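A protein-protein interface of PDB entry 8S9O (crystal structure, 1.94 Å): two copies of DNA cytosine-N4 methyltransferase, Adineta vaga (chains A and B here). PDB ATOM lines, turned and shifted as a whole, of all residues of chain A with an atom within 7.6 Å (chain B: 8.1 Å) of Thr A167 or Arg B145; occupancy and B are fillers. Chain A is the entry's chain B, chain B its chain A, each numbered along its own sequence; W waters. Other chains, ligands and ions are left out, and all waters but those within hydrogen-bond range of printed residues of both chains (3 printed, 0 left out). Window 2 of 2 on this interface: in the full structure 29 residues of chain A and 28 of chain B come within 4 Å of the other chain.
The side-chain hydroxyl (OH) of Tyr A129 sits at hydrogen-bond distance from the backbone carbonyl oxygen (O) of Arg B145, at 2.8 Å.
The backbone carbonyl oxygen (O) of Asn B143 lies within hydrogen-bond range of the guanidinium group (NH1) of Arg A172 (3.3 Å).
The backbone carbonyl oxygen (O) of Tyr B146 is in hydrogen-bond range of the guanidinium group (NH1) of Arg A172 (2.8 Å).
The guanidinium group of Arg A172 lies within hydrogen-bond range of the backbone carbonyl oxygen of Gln B142 (3.3 Å).
The backbone carbonyl oxygen (O) of Phe B147 sits at hydrogen-bond distance from the side-chain amide nitrogen (NE2) of Gln A130 (2.9 Å).
The backbone carbonyl oxygen of Gln A130 is in hydrogen-bond range of the backbone NH of Trp A156 (2.9 Å).
The side-chain amide oxygen (OE1) of Gln B142 is in hydrogen-bond range of the guanidinium group (NE) of Arg B148 (2.9 Å).
The side-chain amide oxygen of Asn B143 is in hydrogen-bond range of the backbone NH of Arg B145, 3.0 Å away.
OG of Ser A100 sits at hydrogen-bond distance from NE1 of Trp A156.
The side-chain hydroxyl of Tyr B146 is in hydrogen-bond range of the side-chain amide nitrogen of Asn B141, at 2.8 Å.
The backbone NH (N) of Asn B143 lies close to the side-chain amide oxygen (OD1) of Asn B141, 3.2 Å away.
Tyr A129 touches Tyr B146.
OE1 of Gln A130 touches CB of Tyr B146 (3.4 Å).
CD2 of Phe B147 touches CZ3 of Trp A156, at 3.5 Å.
Thr A167 touches Arg B145 (OG1 to NH1, 3.7 Å).
Ala B144 touches Phe A170 (O to CD2, 3.4 Å).
Phe A170 touches Arg B145.
Phe A170 touches Tyr B146 (CE2 to C, 3.7 Å).
CZ of Phe A170 touches CE2 of Phe B147, at 3.5 Å.
NH1 of Arg A172 touches CA of Ala B144, at 3.9 Å.
Arg A172 touches Arg B148 (NH1 to CG, 3.5 Å).
Printed residues of chain B within 4 Å of Gln A130: Tyr B146 and Phe B147.
Glu A164 touches none of the printed residues of chain B.
Asn B141 touches none of the printed residues of chain A.
Of the printed residues of chain A, Asn B143 touches Arg A172.
Of the printed residues of chain A, Ala B144 touches Phe A170 and Arg A172.
Of chain A, only Tyr A129 (2.8 Å), Thr A167 (3.7 Å) and Phe A170 (3.6 Å) come within 4 Å of Arg B145.
Of the printed residues of chain A, Arg B148 touches Arg A172.
The nearest residue of chain B that does not touch Thr A167 is Tyr B146 (7.8 Å).
Hydrophobic or aromatic side chains of chain B that line the printed part of chain A: Tyr B146 and Phe B147.
Along chain B the printed residues that touch a printed residue of chain A span positions 142 to 148.
Hydrophobic or aromatic side chains of chain A within 4 Å of the printed part of chain B: Tyr A129, Trp A156 and Phe A170.
Among the printed residues, 15 pairs touch across the chains.
Among the printed residues, no Asp or Glu carboxylate lies within 4 Å of a Lys or Arg side-chain nitrogen of the other chain.
No position is printed for both chains.
Water W1 lies within hydrogen-bond range of the backbone carbonyl oxygen of Ala B144, the backbone NH of Arg A172 and the backbone carbonyl oxygen of Phe A170.
Water W2 lies within hydrogen-bond range of O of Asn B141 (2.7 Å), O of Asn B143 (2.7 Å) and NH1 of Arg A172 (2.9 Å).
Water W3 lies within hydrogen-bond range of the backbone carbonyl oxygen (O) of Pro A168 (2.7 Å), the backbone carbonyl oxygen (O) of Arg B145 (3.1 Å) and the side-chain hydroxyl (OG1) of Thr A167 (3.3 Å).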
ATOM      1  N   PRO A  97       3.252   2.700 -15.472  1.00  0.00           N
ATOM      2  CA  PRO A  97       3.224   2.549 -16.932  1.00  0.00           C
ATOM      3  C   PRO A  97       3.621   3.854 -17.603  1.00  0.00           C
ATOM      4  O   PRO A  97       3.132   4.930 -17.249  1.00  0.00           O
ATOM      5  CB  PRO A  97       1.767   2.175 -17.222  1.00  0.00           C
ATOM      6  CG  PRO A  97       1.295   1.534 -15.959  1.00  0.00           C
ATOM      7  CD  PRO A  97       1.990   2.271 -14.847  1.00  0.00           C
ATOM      8  N   GLY A  98       4.526   3.753 -18.572  1.00  0.00           N
ATOM      9  CA  GLY A  98       5.163   4.924 -19.129  1.00  0.00           C
ATOM     10  C   GLY A  98       6.325   5.456 -18.319  1.00  0.00           C
ATOM     11  O   GLY A  98       6.941   6.446 -18.729  1.00  0.00           O
ATOM     12  N   GLY A  99       6.642   4.836 -17.183  1.00  0.00           N
ATOM     13  CA  GLY A  99       7.766   5.281 -16.389  1.00  0.00           C
ATOM     14  C   GLY A  99       9.097   4.909 -17.014  1.00  0.00           C
ATOM     15  O   GLY A  99       9.191   4.065 -17.906  1.00  0.00           O
ATOM     16  N   SER A 100      10.150   5.558 -16.525  1.00  0.00           N
ATOM     17  CA  SER A 100      11.492   5.373 -17.054  1.00  0.00           C
ATOM     18  C   SER A 100      12.476   5.114 -15.924  1.00  0.00           C
ATOM     19  O   SER A 100      12.340   5.663 -14.827  1.00  0.00           O
ATOM     20  CB  SER A 100      11.948   6.595 -17.859  1.00  0.00           C
ATOM     21  OG  SER A 100      11.258   6.671 -19.094  1.00  0.00           O
ATOM     22  N   TYR A 129      15.237   0.429 -23.690  1.00  0.00           N
ATOM     23  CA  TYR A 129      14.620   1.310 -24.671  1.00  0.00           C
ATOM     24  C   TYR A 129      15.647   2.019 -25.543  1.00  0.00           C
ATOM     25  O   TYR A 129      15.509   2.046 -26.770  1.00  0.00           O
ATOM     26  CB  TYR A 129      13.731   2.337 -23.961  1.00  0.00           C
ATOM     27  CG  TYR A 129      12.922   3.191 -24.904  1.00  0.00           C
ATOM     28  CD1 TYR A 129      11.871   2.645 -25.630  1.00  0.00           C
ATOM     29  CD2 TYR A 129      13.206   4.539 -25.070  1.00  0.00           C
ATOM     30  CE1 TYR A 129      11.126   3.418 -26.499  1.00  0.00           C
ATOM     31  CE2 TYR A 129      12.468   5.322 -25.936  1.00  0.00           C
ATOM     32  CZ  TYR A 129      11.428   4.758 -26.647  1.00  0.00           C
ATOM     33  OH  TYR A 129      10.689   5.536 -27.510  1.00  0.00           O
ATOM     34  N   GLN A 130      16.676   2.593 -24.930  1.00  0.00           N
ATOM     35  CA  GLN A 130      17.755   3.235 -25.664  1.00  0.00           C
ATOM     36  C   GLN A 130      18.982   3.268 -24.767  1.00  0.00           C
ATOM     37  O   GLN A 130      18.867   3.339 -23.540  1.00  0.00           O
ATOM     38  CB  GLN A 130      17.368   4.652 -26.110  1.00  0.00           C
ATOM     39  CG  GLN A 130      18.346   5.292 -27.086  1.00  0.00           C
ATOM     40  CD  GLN A 130      17.897   6.663 -27.552  1.00  0.00           C
ATOM     41  OE1 GLN A 130      17.245   7.401 -26.815  1.00  0.00           O
ATOM     42  NE2 GLN A 130      18.241   7.007 -28.789  1.00  0.00           N
ATOM     43  N   TRP A 156      18.558   3.351 -20.686  1.00  0.00           N
ATOM     44  CA  TRP A 156      17.220   3.897 -20.501  1.00  0.00           C
ATOM     45  C   TRP A 156      16.232   2.741 -20.595  1.00  0.00           C
ATOM     46  O   TRP A 156      15.997   2.201 -21.681  1.00  0.00           O
ATOM     47  CB  TRP A 156      16.946   4.975 -21.549  1.00  0.00           C
ATOM     48  CG  TRP A 156      15.600   5.630 -21.480  1.00  0.00           C
ATOM     49  CD1 TRP A 156      14.641   5.464 -20.522  1.00  0.00           C
ATOM     50  CD2 TRP A 156      15.067   6.565 -22.424  1.00  0.00           C
ATOM     51  NE1 TRP A 156      13.541   6.238 -20.816  1.00  0.00           N
ATOM     52  CE2 TRP A 156      13.779   6.921 -21.979  1.00  0.00           C
ATOM     53  CE3 TRP A 156      15.555   7.133 -23.605  1.00  0.00           C
ATOM     54  CZ2 TRP A 156      12.975   7.824 -22.672  1.00  0.00           C
ATOM     55  CZ3 TRP A 156      14.756   8.026 -24.291  1.00  0.00           C
ATOM     56  CH2 TRP A 156      13.481   8.363 -23.823  1.00  0.00           C
ATOM     57  N   THR A 158      12.312   1.025 -19.697  1.00  0.00           N
ATOM     58  CA  THR A 158      10.902   1.366 -19.610  1.00  0.00           C
ATOM     59  C   THR A 158      10.140   0.141 -19.121  1.00  0.00           C
ATOM     60  O   THR A 158      10.609  -0.994 -19.247  1.00  0.00           O
ATOM     61  CB  THR A 158      10.347   1.856 -20.955  1.00  0.00           C
ATOM     62  OG1 THR A 158       9.032   2.395 -20.753  1.00  0.00           O
ATOM     63  CG2 THR A 158      10.303   0.727 -21.979  1.00  0.00           C
ATOM     64  N   LYS A 159       8.978   0.379 -18.528  1.00  0.00           N
ATOM     65  CA  LYS A 159       8.250  -0.698 -17.879  1.00  0.00           C
ATOM     66  C   LYS A 159       7.574  -1.598 -18.908  1.00  0.00           C
ATOM     67  O   LYS A 159       7.109  -1.139 -19.954  1.00  0.00           O
ATOM     68  CB  LYS A 159       7.205  -0.125 -16.919  1.00  0.00           C
ATOM     69  CG  LYS A 159       6.448  -1.177 -16.112  1.00  0.00           C
ATOM     70  CD  LYS A 159       5.115  -0.635 -15.607  1.00  0.00           C
ATOM     71  CE  LYS A 159       4.348  -1.649 -14.775  1.00  0.00           C
ATOM     72  NZ  LYS A 159       4.869  -1.733 -13.391  1.00  0.00           N
ATOM     73  N   GLU A 164       4.582  -7.003 -22.511  1.00  0.00           N
ATOM     74  CA  GLU A 164       4.400  -6.091 -23.634  1.00  0.00           C
ATOM     75  C   GLU A 164       5.109  -4.769 -23.355  1.00  0.00           C
ATOM     76  O   GLU A 164       5.145  -4.295 -22.214  1.00  0.00           O
ATOM     77  CB  GLU A 164       2.912  -5.842 -23.899  1.00  0.00           C
ATOM     78  N   SER A 165       5.687  -4.190 -24.402  1.00  0.00           N
ATOM     79  CA  SER A 165       6.548  -3.029 -24.251  1.00  0.00           C
ATOM     80  C   SER A 165       5.723  -1.747 -24.259  1.00  0.00           C
ATOM     81  O   SER A 165       4.964  -1.493 -25.201  1.00  0.00           O
ATOM     82  CB  SER A 165       7.586  -2.997 -25.375  1.00  0.00           C
ATOM     83  OG  SER A 165       7.971  -4.298 -25.814  1.00  0.00           O
ATOM     84  N   THR A 166       5.870  -0.936 -23.213  1.00  0.00           N
ATOM     85  CA  THR A 166       5.251   0.379 -23.212  1.00  0.00           C
ATOM     86  C   THR A 166       6.155   1.370 -23.931  1.00  0.00           C
ATOM     87  O   THR A 166       7.287   1.064 -24.312  1.00  0.00           O
ATOM     88  CB  THR A 166       4.962   0.881 -21.794  1.00  0.00           C
ATOM     89  OG1 THR A 166       6.181   0.946 -21.041  1.00  0.00           O
ATOM     90  CG2 THR A 166       3.955  -0.011 -21.087  1.00  0.00           C
ATOM     91  N   THR A 167       5.613   2.565 -24.146  1.00  0.00           N
ATOM     92  CA  THR A 167       6.357   3.702 -24.660  1.00  0.00           C
ATOM     93  C   THR A 167       6.536   4.706 -23.531  1.00  0.00           C
ATOM     94  O   THR A 167       5.544   5.108 -22.903  1.00  0.00           O
ATOM     95  CB  THR A 167       5.628   4.338 -25.847  1.00  0.00           C
ATOM     96  OG1 THR A 167       6.234   5.595 -26.184  1.00  0.00           O
ATOM     97  CG2 THR A 167       4.158   4.544 -25.522  1.00  0.00           C
ATOM     98  N   PRO A 168       7.762   5.106 -23.207  1.00  0.00           N
ATOM     99  CA  PRO A 168       7.960   5.987 -22.051  1.00  0.00           C
ATOM    100  C   PRO A 168       7.410   7.382 -22.302  1.00  0.00           C
ATOM    101  O   PRO A 168       7.515   7.922 -23.406  1.00  0.00           O
ATOM    102  CB  PRO A 168       9.482   6.011 -21.881  1.00  0.00           C
ATOM    103  CG  PRO A 168      10.007   5.728 -23.250  1.00  0.00           C
ATOM    104  CD  PRO A 168       9.032   4.764 -23.868  1.00  0.00           C
ATOM    105  N   LYS A 169       6.795   7.950 -21.267  1.00  0.00           N
ATOM    106  CA  LYS A 169       6.534   9.381 -21.249  1.00  0.00           C
ATOM    107  C   LYS A 169       7.853  10.118 -21.427  1.00  0.00           C
ATOM    108  O   LYS A 169       8.801   9.897 -20.668  1.00  0.00           O
ATOM    109  CB  LYS A 169       5.861   9.774 -19.934  1.00  0.00           C
ATOM    110  CG  LYS A 169       5.740  11.273 -19.683  1.00  0.00           C
ATOM    111  CD  LYS A 169       5.074  11.532 -18.337  1.00  0.00           C
ATOM    112  CE  LYS A 169       5.010  13.015 -17.994  1.00  0.00           C
ATOM    113  NZ  LYS A 169       3.973  13.746 -18.778  1.00  0.00           N
ATOM    114  N   PHE A 170       7.924  10.980 -22.437  1.00  0.00           N
ATOM    115  CA  PHE A 170       9.203  11.581 -22.807  1.00  0.00           C
ATOM    116  C   PHE A 170       8.942  12.884 -23.541  1.00  0.00           C
ATOM    117  O   PHE A 170       8.250  12.891 -24.563  1.00  0.00           O
ATOM    118  CB  PHE A 170      10.016  10.619 -23.673  1.00  0.00           C
ATOM    119  CG  PHE A 170      11.374  11.137 -24.046  1.00  0.00           C
ATOM    120  CD1 PHE A 170      12.306  11.438 -23.068  1.00  0.00           C
ATOM    121  CD2 PHE A 170      11.723  11.308 -25.375  1.00  0.00           C
ATOM    122  CE1 PHE A 170      13.560  11.911 -23.410  1.00  0.00           C
ATOM    123  CE2 PHE A 170      12.974  11.780 -25.723  1.00  0.00           C
ATOM    124  CZ  PHE A 170      13.893  12.082 -24.738  1.00  0.00           C
ATOM    125  N   HIS A 171       9.500  13.980 -23.032  1.00  0.00           N
ATOM    126  CA  HIS A 171       9.303  15.311 -23.602  1.00  0.00           C
ATOM    127  C   HIS A 171      10.672  15.884 -23.950  1.00  0.00           C
ATOM    128  O   HIS A 171      11.259  16.650 -23.183  1.00  0.00           O
ATOM    129  CB  HIS A 171       8.539  16.198 -22.621  1.00  0.00           C
ATOM    130  CG  HIS A 171       7.266  15.585 -22.129  1.00  0.00           C
ATOM    131  ND1 HIS A 171       6.035  15.891 -22.669  1.00  0.00           N
ATOM    132  CD2 HIS A 171       7.032  14.675 -21.154  1.00  0.00           C
ATOM    133  CE1 HIS A 171       5.098  15.199 -22.045  1.00  0.00           C
ATOM    134  NE2 HIS A 171       5.677  14.453 -21.122  1.00  0.00           N
ATOM    135  N   ARG A 172      11.167  15.523 -25.136  1.00  0.00           N
ATOM    136  CA  ARG A 172      12.474  15.984 -25.584  1.00  0.00           C
ATOM    137  C   ARG A 172      12.493  17.484 -25.846  1.00  0.00           C
ATOM    138  O   ARG A 172      13.565  18.095 -25.812  1.00  0.00           O
ATOM    139  CB  ARG A 172      12.883  15.221 -26.843  1.00  0.00           C
ATOM    140  CG  ARG A 172      14.369  15.251 -27.146  1.00  0.00           C
ATOM    141  CD  ARG A 172      14.684  14.423 -28.381  1.00  0.00           C
ATOM    142  NE  ARG A 172      14.293  15.096 -29.613  1.00  0.00           N
ATOM    143  CZ  ARG A 172      14.334  14.534 -30.814  1.00  0.00           C
ATOM    144  NH1 ARG A 172      14.722  13.281 -30.977  1.00  0.00           N
ATOM    145  NH2 ARG A 172      13.976  15.248 -31.878  1.00  0.00           N
ATOM    146  N   ASN B 141      16.290  10.803 -38.757  1.00  0.00           N
ATOM    147  CA  ASN B 141      15.262  10.322 -37.838  1.00  0.00           C
ATOM    148  C   ASN B 141      15.155  11.318 -36.691  1.00  0.00           C
ATOM    149  O   ASN B 141      15.871  11.235 -35.693  1.00  0.00           O
ATOM    150  CB  ASN B 141      15.592   8.921 -37.339  1.00  0.00           C
ATOM    151  CG  ASN B 141      14.524   8.365 -36.418  1.00  0.00           C
ATOM    152  OD1 ASN B 141      13.424   8.909 -36.326  1.00  0.00           O
ATOM    153  ND2 ASN B 141      14.842   7.273 -35.732  1.00  0.00           N
ATOM    154  N   GLN B 142      14.244  12.275 -36.842  1.00  0.00           N
ATOM    155  CA  GLN B 142      13.974  13.271 -35.816  1.00  0.00           C
ATOM    156  C   GLN B 142      12.784  12.898 -34.945  1.00  0.00           C
ATOM    157  O   GLN B 142      12.263  13.757 -34.226  1.00  0.00           O
ATOM    158  CB  GLN B 142      13.749  14.642 -36.455  1.00  0.00           C
ATOM    159  CG  GLN B 142      15.020  15.284 -36.981  1.00  0.00           C
ATOM    160  CD  GLN B 142      16.067  15.467 -35.896  1.00  0.00           C
ATOM    161  OE1 GLN B 142      15.752  15.853 -34.768  1.00  0.00           O
ATOM    162  NE2 GLN B 142      17.319  15.178 -36.229  1.00  0.00           N
ATOM    163  N   ASN B 143      12.334  11.646 -35.011  1.00  0.00           N
ATOM    164  CA  ASN B 143      11.260  11.172 -34.151  1.00  0.00           C
ATOM    165  C   ASN B 143      11.589  11.467 -32.695  1.00  0.00           C
ATOM    166  O   ASN B 143      12.652  11.085 -32.197  1.00  0.00           O
ATOM    167  CB  ASN B 143      11.050   9.671 -34.369  1.00  0.00           C
ATOM    168  CG  ASN B 143       9.764   9.165 -33.754  1.00  0.00           C
ATOM    169  OD1 ASN B 143       9.510   9.364 -32.568  1.00  0.00           O
ATOM    170  ND2 ASN B 143       8.936   8.513 -34.565  1.00  0.00           N
ATOM    171  N   ALA B 144      10.676  12.160 -32.018  1.00  0.00           N
ATOM    172  CA  ALA B 144      10.925  12.695 -30.688  1.00  0.00           C
ATOM    173  C   ALA B 144      10.564  11.719 -29.574  1.00  0.00           C
ATOM    174  O   ALA B 144      10.459  12.131 -28.413  1.00  0.00           O
ATOM    175  CB  ALA B 144      10.169  14.011 -30.500  1.00  0.00           C
ATOM    176  N   ARG B 145      10.369  10.443 -29.898  1.00  0.00           N
ATOM    177  CA  ARG B 145      10.146   9.419 -28.887  1.00  0.00           C
ATOM    178  C   ARG B 145      11.430   8.993 -28.193  1.00  0.00           C
ATOM    179  O   ARG B 145      11.372   8.201 -27.247  1.00  0.00           O
ATOM    180  CB  ARG B 145       9.488   8.188 -29.507  1.00  0.00           C
ATOM    181  CG  ARG B 145       8.072   8.391 -29.997  1.00  0.00           C
ATOM    182  CD  ARG B 145       7.692   7.242 -30.909  1.00  0.00           C
ATOM    183  NE  ARG B 145       6.348   7.377 -31.452  1.00  0.00           N
ATOM    184  CZ  ARG B 145       5.257   6.912 -30.861  1.00  0.00           C
ATOM    185  NH1 ARG B 145       5.316   6.295 -29.692  1.00  0.00           N
ATOM    186  NH2 ARG B 145       4.080   7.070 -31.456  1.00  0.00           N
ATOM    187  N   TYR B 146      12.579   9.482 -28.649  1.00  0.00           N
ATOM    188  CA  TYR B 146      13.865   9.103 -28.085  1.00  0.00           C
ATOM    189  C   TYR B 146      14.870  10.193 -28.419  1.00  0.00           C
ATOM    190  O   TYR B 146      14.587  11.110 -29.192  1.00  0.00           O
ATOM    191  CB  TYR B 146      14.327   7.741 -28.615  1.00  0.00           C
ATOM    192  CG  TYR B 146      13.916   7.464 -30.046  1.00  0.00           C
ATOM    193  CD1 TYR B 146      14.527   8.119 -31.106  1.00  0.00           C
ATOM    194  CD2 TYR B 146      12.921   6.541 -30.335  1.00  0.00           C
ATOM    195  CE1 TYR B 146      14.154   7.865 -32.413  1.00  0.00           C
ATOM    196  CE2 TYR B 146      12.541   6.282 -31.638  1.00  0.00           C
ATOM    197  CZ  TYR B 146      13.161   6.947 -32.672  1.00  0.00           C
ATOM    198  OH  TYR B 146      12.786   6.690 -33.971  1.00  0.00           O
ATOM    199  N   PHE B 147      16.049  10.090 -27.814  1.00  0.00           N
ATOM    200  CA  PHE B 147      17.135  10.992 -28.160  1.00  0.00           C
ATOM    201  C   PHE B 147      17.623  10.690 -29.574  1.00  0.00           C
ATOM    202  O   PHE B 147      17.560   9.551 -30.042  1.00  0.00           O
ATOM    203  CB  PHE B 147      18.269  10.869 -27.144  1.00  0.00           C
ATOM    204  CG  PHE B 147      17.874  11.301 -25.758  1.00  0.00           C
ATOM    205  CD1 PHE B 147      18.021  12.620 -25.366  1.00  0.00           C
ATOM    206  CD2 PHE B 147      17.324  10.398 -24.864  1.00  0.00           C
ATOM    207  CE1 PHE B 147      17.644  13.027 -24.099  1.00  0.00           C
ATOM    208  CE2 PHE B 147      16.947  10.798 -23.595  1.00  0.00           C
ATOM    209  CZ  PHE B 147      17.106  12.115 -23.214  1.00  0.00           C
ATOM    210  N   ARG B 148      18.091  11.730 -30.260  1.00  0.00           N
ATOM    211  CA  ARG B 148      18.446  11.625 -31.669  1.00  0.00           C
ATOM    212  C   ARG B 148      19.467  10.511 -31.877  1.00  0.00           C
ATOM    213  O   ARG B 148      20.574  10.581 -31.321  1.00  0.00           O
ATOM    214  CB  ARG B 148      18.992  12.959 -32.174  1.00  0.00           C
ATOM    215  CG  ARG B 148      17.945  14.065 -32.225  1.00  0.00           C
ATOM    216  CD  ARG B 148      18.575  15.428 -32.455  1.00  0.00           C
ATOM    217  NE  ARG B 148      17.568  16.471 -32.608  1.00  0.00           N
ATOM    218  CZ  ARG B 148      17.805  17.767 -32.461  1.00  0.00           C
ATOM    219  NH1 ARG B 148      19.006  18.218 -32.140  1.00  0.00           N
ATOM    220  NH2 ARG B 148      16.809  18.632 -32.631  1.00  0.00           N
HETATM  221  O   HOH W   1       9.553  13.988 -26.897  1.00  0.00           O
HETATM  222  O   HOH W   2      15.115  11.400 -33.158  1.00  0.00           O
HETATM  223  O   HOH W   3       8.557   7.975 -25.943  1.00  0.00           O
